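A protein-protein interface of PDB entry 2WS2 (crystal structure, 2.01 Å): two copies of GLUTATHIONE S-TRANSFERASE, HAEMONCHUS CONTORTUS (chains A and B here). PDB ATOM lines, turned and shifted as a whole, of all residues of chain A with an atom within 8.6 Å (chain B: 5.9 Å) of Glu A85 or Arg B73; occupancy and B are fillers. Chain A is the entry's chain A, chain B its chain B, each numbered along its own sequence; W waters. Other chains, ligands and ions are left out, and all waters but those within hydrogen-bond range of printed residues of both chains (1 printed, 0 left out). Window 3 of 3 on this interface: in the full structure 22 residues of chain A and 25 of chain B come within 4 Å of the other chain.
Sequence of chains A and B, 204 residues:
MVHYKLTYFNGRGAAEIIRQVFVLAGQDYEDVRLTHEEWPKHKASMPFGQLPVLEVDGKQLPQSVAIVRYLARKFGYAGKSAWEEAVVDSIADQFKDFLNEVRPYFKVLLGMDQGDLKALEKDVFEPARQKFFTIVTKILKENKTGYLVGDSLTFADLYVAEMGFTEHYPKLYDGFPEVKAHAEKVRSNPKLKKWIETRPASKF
Printed residues of chain B within 4 Å of Arg A73: Arg B69, Arg B73 and Glu B85.
Printed residues of chain B within 4 Å of Glu A85: Arg B73.
Printed residues of chain B within 4 Å of Ala A86: Tyr B70 (3.9 Å).
Of the printed residues of chain B, Asp A89 touches Arg B69 (3.3 Å).
Printed residues of chain A within 4 Å of Arg B69: Arg A69 (3.3 Å), Arg A73 (3.6 Å) and Asp A89 (3.3 Å).
Of the printed residues of chain A, Tyr B70 touches Trp A83 and Ala A86.
Arg B73 touches just these residues of chain A: Arg A73 (3.5 Å) and Glu A85 (3.5 Å).
The nearest printed residue of chain B that does not touch Glu A85 is Arg B69 (6.4 Å).
The guanidinium group (NH1) of Arg A73 is in salt-bridge range of the side-chain carboxylate (OE1) of Glu B85 (2.8 Å).
The side-chain carboxylate (OE1) of Glu A85 is in salt-bridge range of the guanidinium group (NH2) of Arg B73, 3.5 Å away.
The guanidinium group (NH1) of Arg B69 lies within salt-bridge range of the side-chain carboxylate (OD2) of Asp A89, at 3.3 Å.
NH1 of Arg A69 lies close to NH2 of Arg B69, 3.3 Å away.
Arg B69 touches Arg A73.
Arg B73 touches Arg A73 (CZ to NH1, 3.5 Å).
Trp A83 touches Tyr B70 (CE3 to CE1, 3.6 Å).
Ala A86 touches Tyr B70 (CB to CD1, 3.9 Å).
Of the 25 printed residues of chain A, 6 touch a printed residue of chain B.
Hydrophobic or aromatic side chains of chain A within 4 Å of the printed part of chain B: Trp A83 and Ala A86.
Hydrophobic or aromatic side chains of chain B that line the printed part of chain A: Tyr B70.
NE of Arg A69 lies within salt-bridge range of OD1 of Asp A89, 2.8 Å away.
The side-chain carboxylate of Glu A85 lies within salt-bridge range of the guanidinium group of Arg A73 (3.6 Å).
The side-chain hydroxyl of Tyr B70 lies within hydrogen-bond range of the side-chain amino group of Lys B74, 3.0 Å away.
OE1 of Glu B85 is in salt-bridge range of NE of Arg B73 (3.1 Å).
Water W1 lies within hydrogen-bond range of OE1 of Glu B85 and NH2 of Arg A73.
Arg A69 touches its own counterpart, Arg B69.
Arg A73 touches Arg B69, but with the chains exchanged Arg A69 does not touch Arg B73 (7.2 Å).
Arg B73 touches its own counterpart, Arg A73.
Arg A73 touches Glu B85, and with the chains exchanged Glu A85 touches Arg B73.
Of the 8 pairs that touch across the chains among the printed residues, 4 have their exchanged pair printed and touching as well.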
ATOM      1  N   ARG A  69      -0.517   3.084  18.365  1.00  0.00           N
ATOM      2  CA  ARG A  69       0.817   3.124  19.036  1.00  0.00           C
ATOM      3  C   ARG A  69       1.761   4.198  18.556  1.00  0.00           C
ATOM      4  O   ARG A  69       2.447   4.841  19.376  1.00  0.00           O
ATOM      5  CB  ARG A  69       1.502   1.758  19.044  1.00  0.00           C
ATOM      6  CG  ARG A  69       2.784   1.693  19.861  1.00  0.00           C
ATOM      7  CD  ARG A  69       3.292   0.286  19.901  1.00  0.00           C
ATOM      8  NE  ARG A  69       2.227  -0.634  20.191  1.00  0.00           N
ATOM      9  CZ  ARG A  69       1.656  -1.476  19.339  1.00  0.00           C
ATOM     10  NH1 ARG A  69       2.024  -1.544  18.040  1.00  0.00           N
ATOM     11  NH2 ARG A  69       0.692  -2.255  19.808  1.00  0.00           N
ATOM     12  N   ALA A  72       0.283   7.756  19.596  1.00  0.00           N
ATOM     13  CA  ALA A  72       0.308   7.778  21.073  1.00  0.00           C
ATOM     14  C   ALA A  72       1.702   8.052  21.686  1.00  0.00           C
ATOM     15  O   ALA A  72       1.838   8.886  22.592  1.00  0.00           O
ATOM     16  CB  ALA A  72      -0.269   6.472  21.598  1.00  0.00           C
ATOM     17  N   ARG A  73       2.730   7.355  21.157  1.00  0.00           N
ATOM     18  CA  ARG A  73       4.136   7.594  21.498  1.00  0.00           C
ATOM     19  C   ARG A  73       4.565   9.014  21.236  1.00  0.00           C
ATOM     20  O   ARG A  73       5.134   9.664  22.101  1.00  0.00           O
ATOM     21  CB  ARG A  73       5.069   6.678  20.674  1.00  0.00           C
ATOM     22  CG  ARG A  73       5.310   5.360  21.295  1.00  0.00           C
ATOM     23  CD  ARG A  73       6.454   4.619  20.603  1.00  0.00           C
ATOM     24  NE  ARG A  73       6.377   3.204  20.916  1.00  0.00           N
ATOM     25  CZ  ARG A  73       7.226   2.290  20.472  1.00  0.00           C
ATOM     26  NH1 ARG A  73       8.259   2.644  19.680  1.00  0.00           N
ATOM     27  NH2 ARG A  73       7.042   1.030  20.821  1.00  0.00           N
ATOM     28  N   LYS A  74       4.307   9.509  20.038  1.00  0.00           N
ATOM     29  CA  LYS A  74       4.789  10.849  19.697  1.00  0.00           C
ATOM     30  C   LYS A  74       4.067  11.934  20.505  1.00  0.00           C
ATOM     31  O   LYS A  74       4.631  12.990  20.744  1.00  0.00           O
ATOM     32  CB  LYS A  74       4.729  11.129  18.174  1.00  0.00           C
ATOM     33  CG  LYS A  74       3.363  11.412  17.600  1.00  0.00           C
ATOM     34  CD  LYS A  74       3.329  11.412  16.065  1.00  0.00           C
ATOM     35  CE  LYS A  74       4.026  12.586  15.460  1.00  0.00           C
ATOM     36  NZ  LYS A  74       4.300  12.279  14.025  1.00  0.00           N
ATOM     37  N   GLY A  76       2.314  11.275  23.779  1.00  0.00           N
ATOM     38  CA  GLY A  76       2.377  11.072  25.253  1.00  0.00           C
ATOM     39  C   GLY A  76       1.206  10.312  25.878  1.00  0.00           C
ATOM     40  O   GLY A  76       0.794  10.571  27.040  1.00  0.00           O
ATOM     41  N   TYR A  77       0.681   9.349  25.131  1.00  0.00           N
ATOM     42  CA  TYR A  77      -0.475   8.583  25.571  1.00  0.00           C
ATOM     43  C   TYR A  77      -0.264   7.090  25.352  1.00  0.00           C
ATOM     44  O   TYR A  77      -1.214   6.322  25.293  1.00  0.00           O
ATOM     45  CB  TYR A  77      -1.732   9.055  24.827  1.00  0.00           C
ATOM     46  CG  TYR A  77      -2.124  10.468  25.115  1.00  0.00           C
ATOM     47  CD1 TYR A  77      -1.837  11.493  24.216  1.00  0.00           C
ATOM     48  CD2 TYR A  77      -2.795  10.788  26.293  1.00  0.00           C
ATOM     49  CE1 TYR A  77      -2.233  12.801  24.476  1.00  0.00           C
ATOM     50  CE2 TYR A  77      -3.176  12.085  26.573  1.00  0.00           C
ATOM     51  CZ  TYR A  77      -2.901  13.080  25.685  1.00  0.00           C
ATOM     52  OH  TYR A  77      -3.299  14.355  25.981  1.00  0.00           O
ATOM     53  N   ALA A  78       1.005   6.690  25.330  1.00  0.00           N
ATOM     54  CA  ALA A  78       1.410   5.303  25.081  1.00  0.00           C
ATOM     55  C   ALA A  78       1.861   4.614  26.358  1.00  0.00           C
ATOM     56  O   ALA A  78       2.125   3.404  26.340  1.00  0.00           O
ATOM     57  CB  ALA A  78       2.558   5.260  24.010  1.00  0.00           C
ATOM     58  N   GLY A  79       1.941   5.398  27.446  1.00  0.00           N
ATOM     59  CA  GLY A  79       2.536   4.999  28.743  1.00  0.00           C
ATOM     60  C   GLY A  79       3.690   5.897  29.206  1.00  0.00           C
ATOM     61  O   GLY A  79       4.409   6.488  28.380  1.00  0.00           O
ATOM     62  N   LYS A  80       3.908   6.014  30.517  1.00  0.00           N
ATOM     63  CA  LYS A  80       4.916   6.997  31.008  1.00  0.00           C
ATOM     64  C   LYS A  80       6.366   6.487  31.170  1.00  0.00           C
ATOM     65  O   LYS A  80       7.280   7.272  31.374  1.00  0.00           O
ATOM     66  CB  LYS A  80       4.425   7.721  32.281  1.00  0.00           C
ATOM     67  CG  LYS A  80       3.271   8.690  31.980  1.00  0.00           C
ATOM     68  CD  LYS A  80       3.745   9.901  31.167  1.00  0.00           C
ATOM     69  CE  LYS A  80       2.637  10.406  30.230  1.00  0.00           C
ATOM     70  NZ  LYS A  80       2.847  11.761  29.577  1.00  0.00           N
ATOM     71  N   SER A  81       6.568   5.194  31.053  1.00  0.00           N
ATOM     72  CA  SER A  81       7.910   4.644  31.080  1.00  0.00           C
ATOM     73  C   SER A  81       7.862   3.511  30.076  1.00  0.00           C
ATOM     74  O   SER A  81       6.769   3.105  29.664  1.00  0.00           O
ATOM     75  CB  SER A  81       8.188   4.081  32.459  1.00  0.00           C
ATOM     76  OG  SER A  81       7.368   2.958  32.640  1.00  0.00           O
ATOM     77  N   ALA A  82       9.013   2.957  29.735  1.00  0.00           N
ATOM     78  CA  ALA A  82       9.067   1.944  28.666  1.00  0.00           C
ATOM     79  C   ALA A  82       8.381   0.666  29.114  1.00  0.00           C
ATOM     80  O   ALA A  82       7.688   0.026  28.318  1.00  0.00           O
ATOM     81  CB  ALA A  82      10.531   1.698  28.166  1.00  0.00           C
ATOM     82  N   TRP A  83       8.509   0.323  30.406  1.00  0.00           N
ATOM     83  CA  TRP A  83       7.796  -0.827  30.967  1.00  0.00           C
ATOM     84  C   TRP A  83       6.275  -0.629  30.917  1.00  0.00           C
ATOM     85  O   TRP A  83       5.528  -1.581  30.597  1.00  0.00           O
ATOM     86  CB  TRP A  83       8.314  -1.207  32.389  1.00  0.00           C
ATOM     87  CG  TRP A  83       7.414  -2.162  33.085  1.00  0.00           C
ATOM     88  CD1 TRP A  83       6.400  -1.842  33.950  1.00  0.00           C
ATOM     89  CD2 TRP A  83       7.403  -3.584  32.961  1.00  0.00           C
ATOM     90  NE1 TRP A  83       5.764  -2.967  34.371  1.00  0.00           N
ATOM     91  CE2 TRP A  83       6.331  -4.056  33.760  1.00  0.00           C
ATOM     92  CE3 TRP A  83       8.194  -4.509  32.260  1.00  0.00           C
ATOM     93  CZ2 TRP A  83       6.053  -5.410  33.910  1.00  0.00           C
ATOM     94  CZ3 TRP A  83       7.888  -5.861  32.369  1.00  0.00           C
ATOM     95  CH2 TRP A  83       6.841  -6.308  33.178  1.00  0.00           C
ATOM     96  N   GLU A  84       5.837   0.600  31.203  1.00  0.00           N
ATOM     97  CA  GLU A  84       4.416   1.000  31.183  1.00  0.00           C
ATOM     98  C   GLU A  84       3.885   0.910  29.737  1.00  0.00           C
ATOM     99  O   GLU A  84       2.729   0.538  29.517  1.00  0.00           O
ATOM    100  CB  GLU A  84       4.254   2.433  31.750  1.00  0.00           C
ATOM    101  CG  GLU A  84       2.804   2.996  31.839  1.00  0.00           C
ATOM    102  CD  GLU A  84       2.674   4.228  32.752  1.00  0.00           C
ATOM    103  OE1 GLU A  84       2.196   5.285  32.266  1.00  0.00           O
ATOM    104  OE2 GLU A  84       3.073   4.150  33.956  1.00  0.00           O
ATOM    105  N   GLU A  85       4.750   1.180  28.764  1.00  0.00           N
ATOM    106  CA  GLU A  85       4.305   1.192  27.372  1.00  0.00           C
ATOM    107  C   GLU A  85       4.005  -0.220  26.917  1.00  0.00           C
ATOM    108  O   GLU A  85       3.203  -0.441  26.026  1.00  0.00           O
ATOM    109  CB  GLU A  85       5.355   1.817  26.479  1.00  0.00           C
ATOM    110  CG  GLU A  85       5.493   3.282  26.669  1.00  0.00           C
ATOM    111  CD  GLU A  85       6.521   3.883  25.756  1.00  0.00           C
ATOM    112  OE1 GLU A  85       6.382   3.791  24.514  1.00  0.00           O
ATOM    113  OE2 GLU A  85       7.474   4.473  26.297  1.00  0.00           O
ATOM    114  N   ALA A  86       4.649  -1.179  27.542  1.00  0.00           N
ATOM    115  CA  ALA A  86       4.480  -2.555  27.117  1.00  0.00           C
ATOM    116  C   ALA A  86       3.284  -3.052  27.865  1.00  0.00           C
ATOM    117  O   ALA A  86       2.546  -3.885  27.400  1.00  0.00           O
ATOM    118  CB  ALA A  86       5.685  -3.379  27.460  1.00  0.00           C
ATOM    119  N   VAL A  87       3.144  -2.585  29.083  1.00  0.00           N
ATOM    120  CA  VAL A  87       1.940  -2.947  29.863  1.00  0.00           C
ATOM    121  C   VAL A  87       0.671  -2.547  29.084  1.00  0.00           C
ATOM    122  O   VAL A  87      -0.253  -3.328  28.916  1.00  0.00           O
ATOM    123  CB  VAL A  87       2.003  -2.343  31.290  1.00  0.00           C
ATOM    124  CG1 VAL A  87       0.561  -2.110  31.880  1.00  0.00           C
ATOM    125  CG2 VAL A  87       2.880  -3.213  32.240  1.00  0.00           C
ATOM    126  N   VAL A  88       0.662  -1.305  28.647  1.00  0.00           N
ATOM    127  CA  VAL A  88      -0.326  -0.648  27.797  1.00  0.00           C
ATOM    128  C   VAL A  88      -0.578  -1.451  26.532  1.00  0.00           C
ATOM    129  O   VAL A  88      -1.738  -1.765  26.214  1.00  0.00           O
ATOM    130  CB  VAL A  88       0.214   0.713  27.360  1.00  0.00           C
ATOM    131  CG1 VAL A  88      -0.448   1.197  26.037  1.00  0.00           C
ATOM    132  CG2 VAL A  88       0.019   1.772  28.465  1.00  0.00           C
ATOM    133  N   ASP A  89       0.525  -1.840  25.868  1.00  0.00           N
ATOM    134  CA  ASP A  89       0.434  -2.725  24.749  1.00  0.00           C
ATOM    135  C   ASP A  89      -0.277  -3.998  25.170  1.00  0.00           C
ATOM    136  O   ASP A  89      -1.176  -4.363  24.516  1.00  0.00           O
ATOM    137  CB  ASP A  89       1.847  -3.046  24.135  1.00  0.00           C
ATOM    138  CG  ASP A  89       2.399  -1.891  23.296  1.00  0.00           C
ATOM    139  OD1 ASP A  89       1.616  -0.980  22.902  1.00  0.00           O
ATOM    140  OD2 ASP A  89       3.623  -1.869  22.980  1.00  0.00           O
ATOM    141  N   SER A  90       0.095  -4.640  26.283  1.00  0.00           N
ATOM    142  CA  SER A  90      -0.418  -5.983  26.600  1.00  0.00           C
ATOM    143  C   SER A  90      -1.925  -5.964  26.870  1.00  0.00           C
ATOM    144  O   SER A  90      -2.627  -6.944  26.613  1.00  0.00           O
ATOM    145  CB  SER A  90       0.299  -6.586  27.835  1.00  0.00           C
ATOM    146  OG  SER A  90      -0.242  -6.011  29.052  1.00  0.00           O
ATOM    147  N   ILE A  91      -2.389  -4.870  27.464  1.00  0.00           N
ATOM    148  CA  ILE A  91      -3.863  -4.658  27.709  1.00  0.00           C
ATOM    149  C   ILE A  91      -4.698  -4.375  26.413  1.00  0.00           C
ATOM    150  O   ILE A  91      -5.684  -5.027  26.164  1.00  0.00           O
ATOM    151  CB  ILE A  91      -4.134  -3.570  28.784  1.00  0.00           C
ATOM    152  CG1 ILE A  91      -3.467  -3.989  30.103  1.00  0.00           C
ATOM    153  CG2 ILE A  91      -5.688  -3.392  28.984  1.00  0.00           C
ATOM    154  CD1 ILE A  91      -3.545  -2.976  31.254  1.00  0.00           C
ATOM    155  N   ALA A  92      -4.258  -3.435  25.583  1.00  0.00           N
ATOM    156  CA  ALA A  92      -4.764  -3.309  24.181  1.00  0.00           C
ATOM    157  C   ALA A  92      -4.795  -4.609  23.351  1.00  0.00           C
ATOM    158  O   ALA A  92      -5.641  -4.787  22.473  1.00  0.00           O
ATOM    159  CB  ALA A  92      -3.989  -2.240  23.419  1.00  0.00           C
ATOM    160  N   VAL A 149      -3.277   2.234  33.821  1.00  0.00           N
ATOM    161  CA  VAL A 149      -1.811   2.154  33.805  1.00  0.00           C
ATOM    162  C   VAL A 149      -1.311   3.570  34.105  1.00  0.00           C
ATOM    163  O   VAL A 149      -1.712   4.537  33.467  1.00  0.00           O
ATOM    164  CB  VAL A 149      -1.309   1.631  32.404  1.00  0.00           C
ATOM    165  CG1 VAL A 149       0.201   1.560  32.346  1.00  0.00           C
ATOM    166  CG2 VAL A 149      -1.916   0.280  32.099  1.00  0.00           C
ATOM    167  N   THR A 154      -3.956   6.659  28.801  1.00  0.00           N
ATOM    168  CA  THR A 154      -3.204   5.958  27.727  1.00  0.00           C
ATOM    169  C   THR A 154      -4.172   5.395  26.661  1.00  0.00           C
ATOM    170  O   THR A 154      -5.386   5.465  26.869  1.00  0.00           O
ATOM    171  CB  THR A 154      -2.301   4.893  28.370  1.00  0.00           C
ATOM    172  OG1 THR A 154      -1.269   4.492  27.442  1.00  0.00           O
ATOM    173  CG2 THR A 154      -3.123   3.698  28.832  1.00  0.00           C
ATOM    174  N   PHE A 155      -3.695   4.817  25.532  1.00  0.00           N
ATOM    175  CA  PHE A 155      -4.648   4.407  24.479  1.00  0.00           C
ATOM    176  C   PHE A 155      -5.306   3.119  24.909  1.00  0.00           C
ATOM    177  O   PHE A 155      -6.364   2.742  24.369  1.00  0.00           O
ATOM    178  CB  PHE A 155      -4.022   4.271  23.042  1.00  0.00           C
ATOM    179  CG  PHE A 155      -2.923   3.225  22.948  1.00  0.00           C
ATOM    180  CD1 PHE A 155      -1.596   3.590  23.135  1.00  0.00           C
ATOM    181  CD2 PHE A 155      -3.216   1.889  22.712  1.00  0.00           C
ATOM    182  CE1 PHE A 155      -0.563   2.639  23.092  1.00  0.00           C
ATOM    183  CE2 PHE A 155      -2.186   0.921  22.642  1.00  0.00           C
ATOM    184  CZ  PHE A 155      -0.859   1.311  22.841  1.00  0.00           C
ATOM    185  N   ALA A 156      -4.718   2.471  25.916  1.00  0.00           N
ATOM    186  CA  ALA A 156      -5.320   1.272  26.492  1.00  0.00           C
ATOM    187  C   ALA A 156      -6.677   1.591  27.173  1.00  0.00           C
ATOM    188  O   ALA A 156      -7.620   0.795  27.100  1.00  0.00           O
ATOM    189  CB  ALA A 156      -4.404   0.629  27.441  1.00  0.00           C
ATOM    190  N   VAL B  68       7.224  -9.584  22.783  1.00  0.00           N
ATOM    191  CA  VAL B  68       8.132  -9.467  21.602  1.00  0.00           C
ATOM    192  C   VAL B  68       8.611  -8.053  21.425  1.00  0.00           C
ATOM    193  O   VAL B  68       9.818  -7.830  21.321  1.00  0.00           O
ATOM    194  CB  VAL B  68       7.499 -10.005  20.292  1.00  0.00           C
ATOM    195  CG1 VAL B  68       8.424  -9.761  19.075  1.00  0.00           C
ATOM    196  CG2 VAL B  68       7.239 -11.462  20.427  1.00  0.00           C
ATOM    197  N   ARG B  69       7.688  -7.074  21.436  1.00  0.00           N
ATOM    198  CA  ARG B  69       8.095  -5.700  21.205  1.00  0.00           C
ATOM    199  C   ARG B  69       8.963  -5.124  22.302  1.00  0.00           C
ATOM    200  O   ARG B  69       9.876  -4.349  21.998  1.00  0.00           O
ATOM    201  CB  ARG B  69       6.880  -4.774  20.882  1.00  0.00           C
ATOM    202  CG  ARG B  69       7.148  -3.255  20.930  1.00  0.00           C
ATOM    203  CD  ARG B  69       5.908  -2.388  20.532  1.00  0.00           C
ATOM    204  NE  ARG B  69       5.235  -2.989  19.387  1.00  0.00           N
ATOM    205  CZ  ARG B  69       4.177  -3.801  19.455  1.00  0.00           C
ATOM    206  NH1 ARG B  69       3.591  -4.116  20.625  1.00  0.00           N
ATOM    207  NH2 ARG B  69       3.726  -4.325  18.326  1.00  0.00           N
ATOM    208  N   TYR B  70       8.647  -5.469  23.565  1.00  0.00           N
ATOM    209  CA  TYR B  70       9.378  -4.991  24.754  1.00  0.00           C
ATOM    210  C   TYR B  70      10.839  -5.424  24.620  1.00  0.00           C
ATOM    211  O   TYR B  70      11.767  -4.613  24.737  1.00  0.00           O
ATOM    212  CB  TYR B  70       8.768  -5.609  26.016  1.00  0.00           C
ATOM    213  CG  TYR B  70       9.552  -5.419  27.299  1.00  0.00           C
ATOM    214  CD1 TYR B  70       9.425  -4.243  28.062  1.00  0.00           C
ATOM    215  CD2 TYR B  70      10.403  -6.427  27.773  1.00  0.00           C
ATOM    216  CE1 TYR B  70      10.130  -4.071  29.233  1.00  0.00           C
ATOM    217  CE2 TYR B  70      11.117  -6.257  28.952  1.00  0.00           C
ATOM    218  CZ  TYR B  70      10.971  -5.069  29.672  1.00  0.00           C
ATOM    219  OH  TYR B  70      11.653  -4.917  30.854  1.00  0.00           O
ATOM    220  N   LEU B  71      11.008  -6.690  24.308  1.00  0.00           N
ATOM    221  CA  LEU B  71      12.359  -7.243  24.112  1.00  0.00           C
ATOM    222  C   LEU B  71      13.124  -6.660  22.944  1.00  0.00           C
ATOM    223  O   LEU B  71      14.291  -6.272  23.101  1.00  0.00           O
ATOM    224  CB  LEU B  71      12.335  -8.766  24.047  1.00  0.00           C
ATOM    225  CG  LEU B  71      11.744  -9.361  25.317  1.00  0.00           C
ATOM    226  CD1 LEU B  71      11.683 -10.835  25.256  1.00  0.00           C
ATOM    227  CD2 LEU B  71      12.507  -8.910  26.583  1.00  0.00           C
ATOM    228  N   ALA B  72      12.479  -6.556  21.791  1.00  0.00           N
ATOM    229  CA  ALA B  72      13.192  -6.087  20.582  1.00  0.00           C
ATOM    230  C   ALA B  72      13.588  -4.621  20.775  1.00  0.00           C
ATOM    231  O   ALA B  72      14.653  -4.164  20.317  1.00  0.00           O
ATOM    232  CB  ALA B  72      12.291  -6.265  19.353  1.00  0.00           C
ATOM    233  N   ARG B  73      12.718  -3.883  21.477  1.00  0.00           N
ATOM    234  CA  ARG B  73      12.974  -2.480  21.773  1.00  0.00           C
ATOM    235  C   ARG B  73      14.240  -2.299  22.577  1.00  0.00           C
ATOM    236  O   ARG B  73      15.029  -1.384  22.315  1.00  0.00           O
ATOM    237  CB  ARG B  73      11.817  -1.864  22.594  1.00  0.00           C
ATOM    238  CG  ARG B  73      10.697  -1.324  21.752  1.00  0.00           C
ATOM    239  CD  ARG B  73      10.002  -0.145  22.442  1.00  0.00           C
ATOM    240  NE  ARG B  73      10.656   1.087  22.036  1.00  0.00           N
ATOM    241  CZ  ARG B  73      10.357   2.309  22.487  1.00  0.00           C
ATOM    242  NH1 ARG B  73      11.022   3.353  22.021  1.00  0.00           N
ATOM    243  NH2 ARG B  73       9.401   2.488  23.400  1.00  0.00           N
ATOM    244  N   LYS B  74      14.387  -3.162  23.575  1.00  0.00           N
ATOM    245  CA  LYS B  74      15.485  -3.136  24.530  1.00  0.00           C
ATOM    246  C   LYS B  74      16.766  -3.628  23.811  1.00  0.00           C
ATOM    247  O   LYS B  74      17.804  -2.988  23.899  1.00  0.00           O
ATOM    248  CB  LYS B  74      15.140  -4.008  25.734  1.00  0.00           C
ATOM    249  CG  LYS B  74      16.096  -3.913  26.924  1.00  0.00           C
ATOM    250  CD  LYS B  74      15.885  -5.042  27.944  1.00  0.00           C
ATOM    251  CE  LYS B  74      14.629  -4.834  28.760  1.00  0.00           C
ATOM    252  NZ  LYS B  74      14.414  -5.716  29.957  1.00  0.00           N
ATOM    253  N   PHE B  75      16.643  -4.707  23.038  1.00  0.00           N
ATOM    254  CA  PHE B  75      17.819  -5.333  22.394  1.00  0.00           C
ATOM    255  C   PHE B  75      18.182  -4.827  21.002  1.00  0.00           C
ATOM    256  O   PHE B  75      19.179  -5.287  20.390  1.00  0.00           O
ATOM    257  CB  PHE B  75      17.649  -6.853  22.419  1.00  0.00           C
ATOM    258  CG  PHE B  75      17.626  -7.413  23.801  1.00  0.00           C
ATOM    259  CD1 PHE B  75      16.597  -8.244  24.217  1.00  0.00           C
ATOM    260  CD2 PHE B  75      18.614  -7.064  24.719  1.00  0.00           C
ATOM    261  CE1 PHE B  75      16.564  -8.745  25.495  1.00  0.00           C
ATOM    262  CE2 PHE B  75      18.597  -7.592  26.022  1.00  0.00           C
ATOM    263  CZ  PHE B  75      17.567  -8.429  26.410  1.00  0.00           C
ATOM    264  N   GLY B  76      17.403  -3.867  20.521  1.00  0.00           N
ATOM    265  CA  GLY B  76      17.602  -3.218  19.208  1.00  0.00           C
ATOM    266  C   GLY B  76      17.122  -3.888  17.915  1.00  0.00           C
ATOM    267  O   GLY B  76      17.599  -3.506  16.843  1.00  0.00           O
ATOM    268  N   TYR B  77      16.153  -4.819  18.014  1.00  0.00           N
ATOM    269  CA  TYR B  77      15.505  -5.480  16.838  1.00  0.00           C
ATOM    270  C   TYR B  77      14.001  -5.085  16.579  1.00  0.00           C
ATOM    271  O   TYR B  77      13.123  -5.906  16.232  1.00  0.00           O
ATOM    272  CB  TYR B  77      15.664  -6.995  16.934  1.00  0.00           C
ATOM    273  CG  TYR B  77      17.117  -7.501  17.148  1.00  0.00           C
ATOM    274  CD1 TYR B  77      17.637  -7.715  18.439  1.00  0.00           C
ATOM    275  CD2 TYR B  77      17.938  -7.801  16.059  1.00  0.00           C
ATOM    276  CE1 TYR B  77      18.955  -8.232  18.631  1.00  0.00           C
ATOM    277  CE2 TYR B  77      19.254  -8.294  16.234  1.00  0.00           C
ATOM    278  CZ  TYR B  77      19.758  -8.499  17.506  1.00  0.00           C
ATOM    279  OH  TYR B  77      21.053  -8.981  17.655  1.00  0.00           O
ATOM    280  N   ALA B  78      13.695  -3.818  16.746  1.00  0.00           N
ATOM    281  CA  ALA B  78      12.286  -3.406  16.674  1.00  0.00           C
ATOM    282  C   ALA B  78      12.119  -2.437  15.549  1.00  0.00           C
ATOM    283  O   ALA B  78      11.001  -2.008  15.245  1.00  0.00           O
ATOM    284  CB  ALA B  78      11.786  -2.803  18.030  1.00  0.00           C
ATOM    285  N   GLU B  85      10.115   1.731  13.497  1.00  0.00           N
ATOM    286  CA  GLU B  85       9.537   0.865  14.493  1.00  0.00           C
ATOM    287  C   GLU B  85       8.087   0.547  14.105  1.00  0.00           C
ATOM    288  O   GLU B  85       7.641  -0.588  14.272  1.00  0.00           O
ATOM    289  CB  GLU B  85       9.635   1.432  15.950  1.00  0.00           C
ATOM    290  CG  GLU B  85      11.068   1.449  16.594  1.00  0.00           C
ATOM    291  CD  GLU B  85      11.081   1.968  18.034  1.00  0.00           C
ATOM    292  OE1 GLU B  85      10.588   1.247  18.937  1.00  0.00           O
ATOM    293  OE2 GLU B  85      11.597   3.097  18.271  1.00  0.00           O
HETATM  294  O   HOH W   1       8.932  -0.577  18.931  1.00  0.00           O
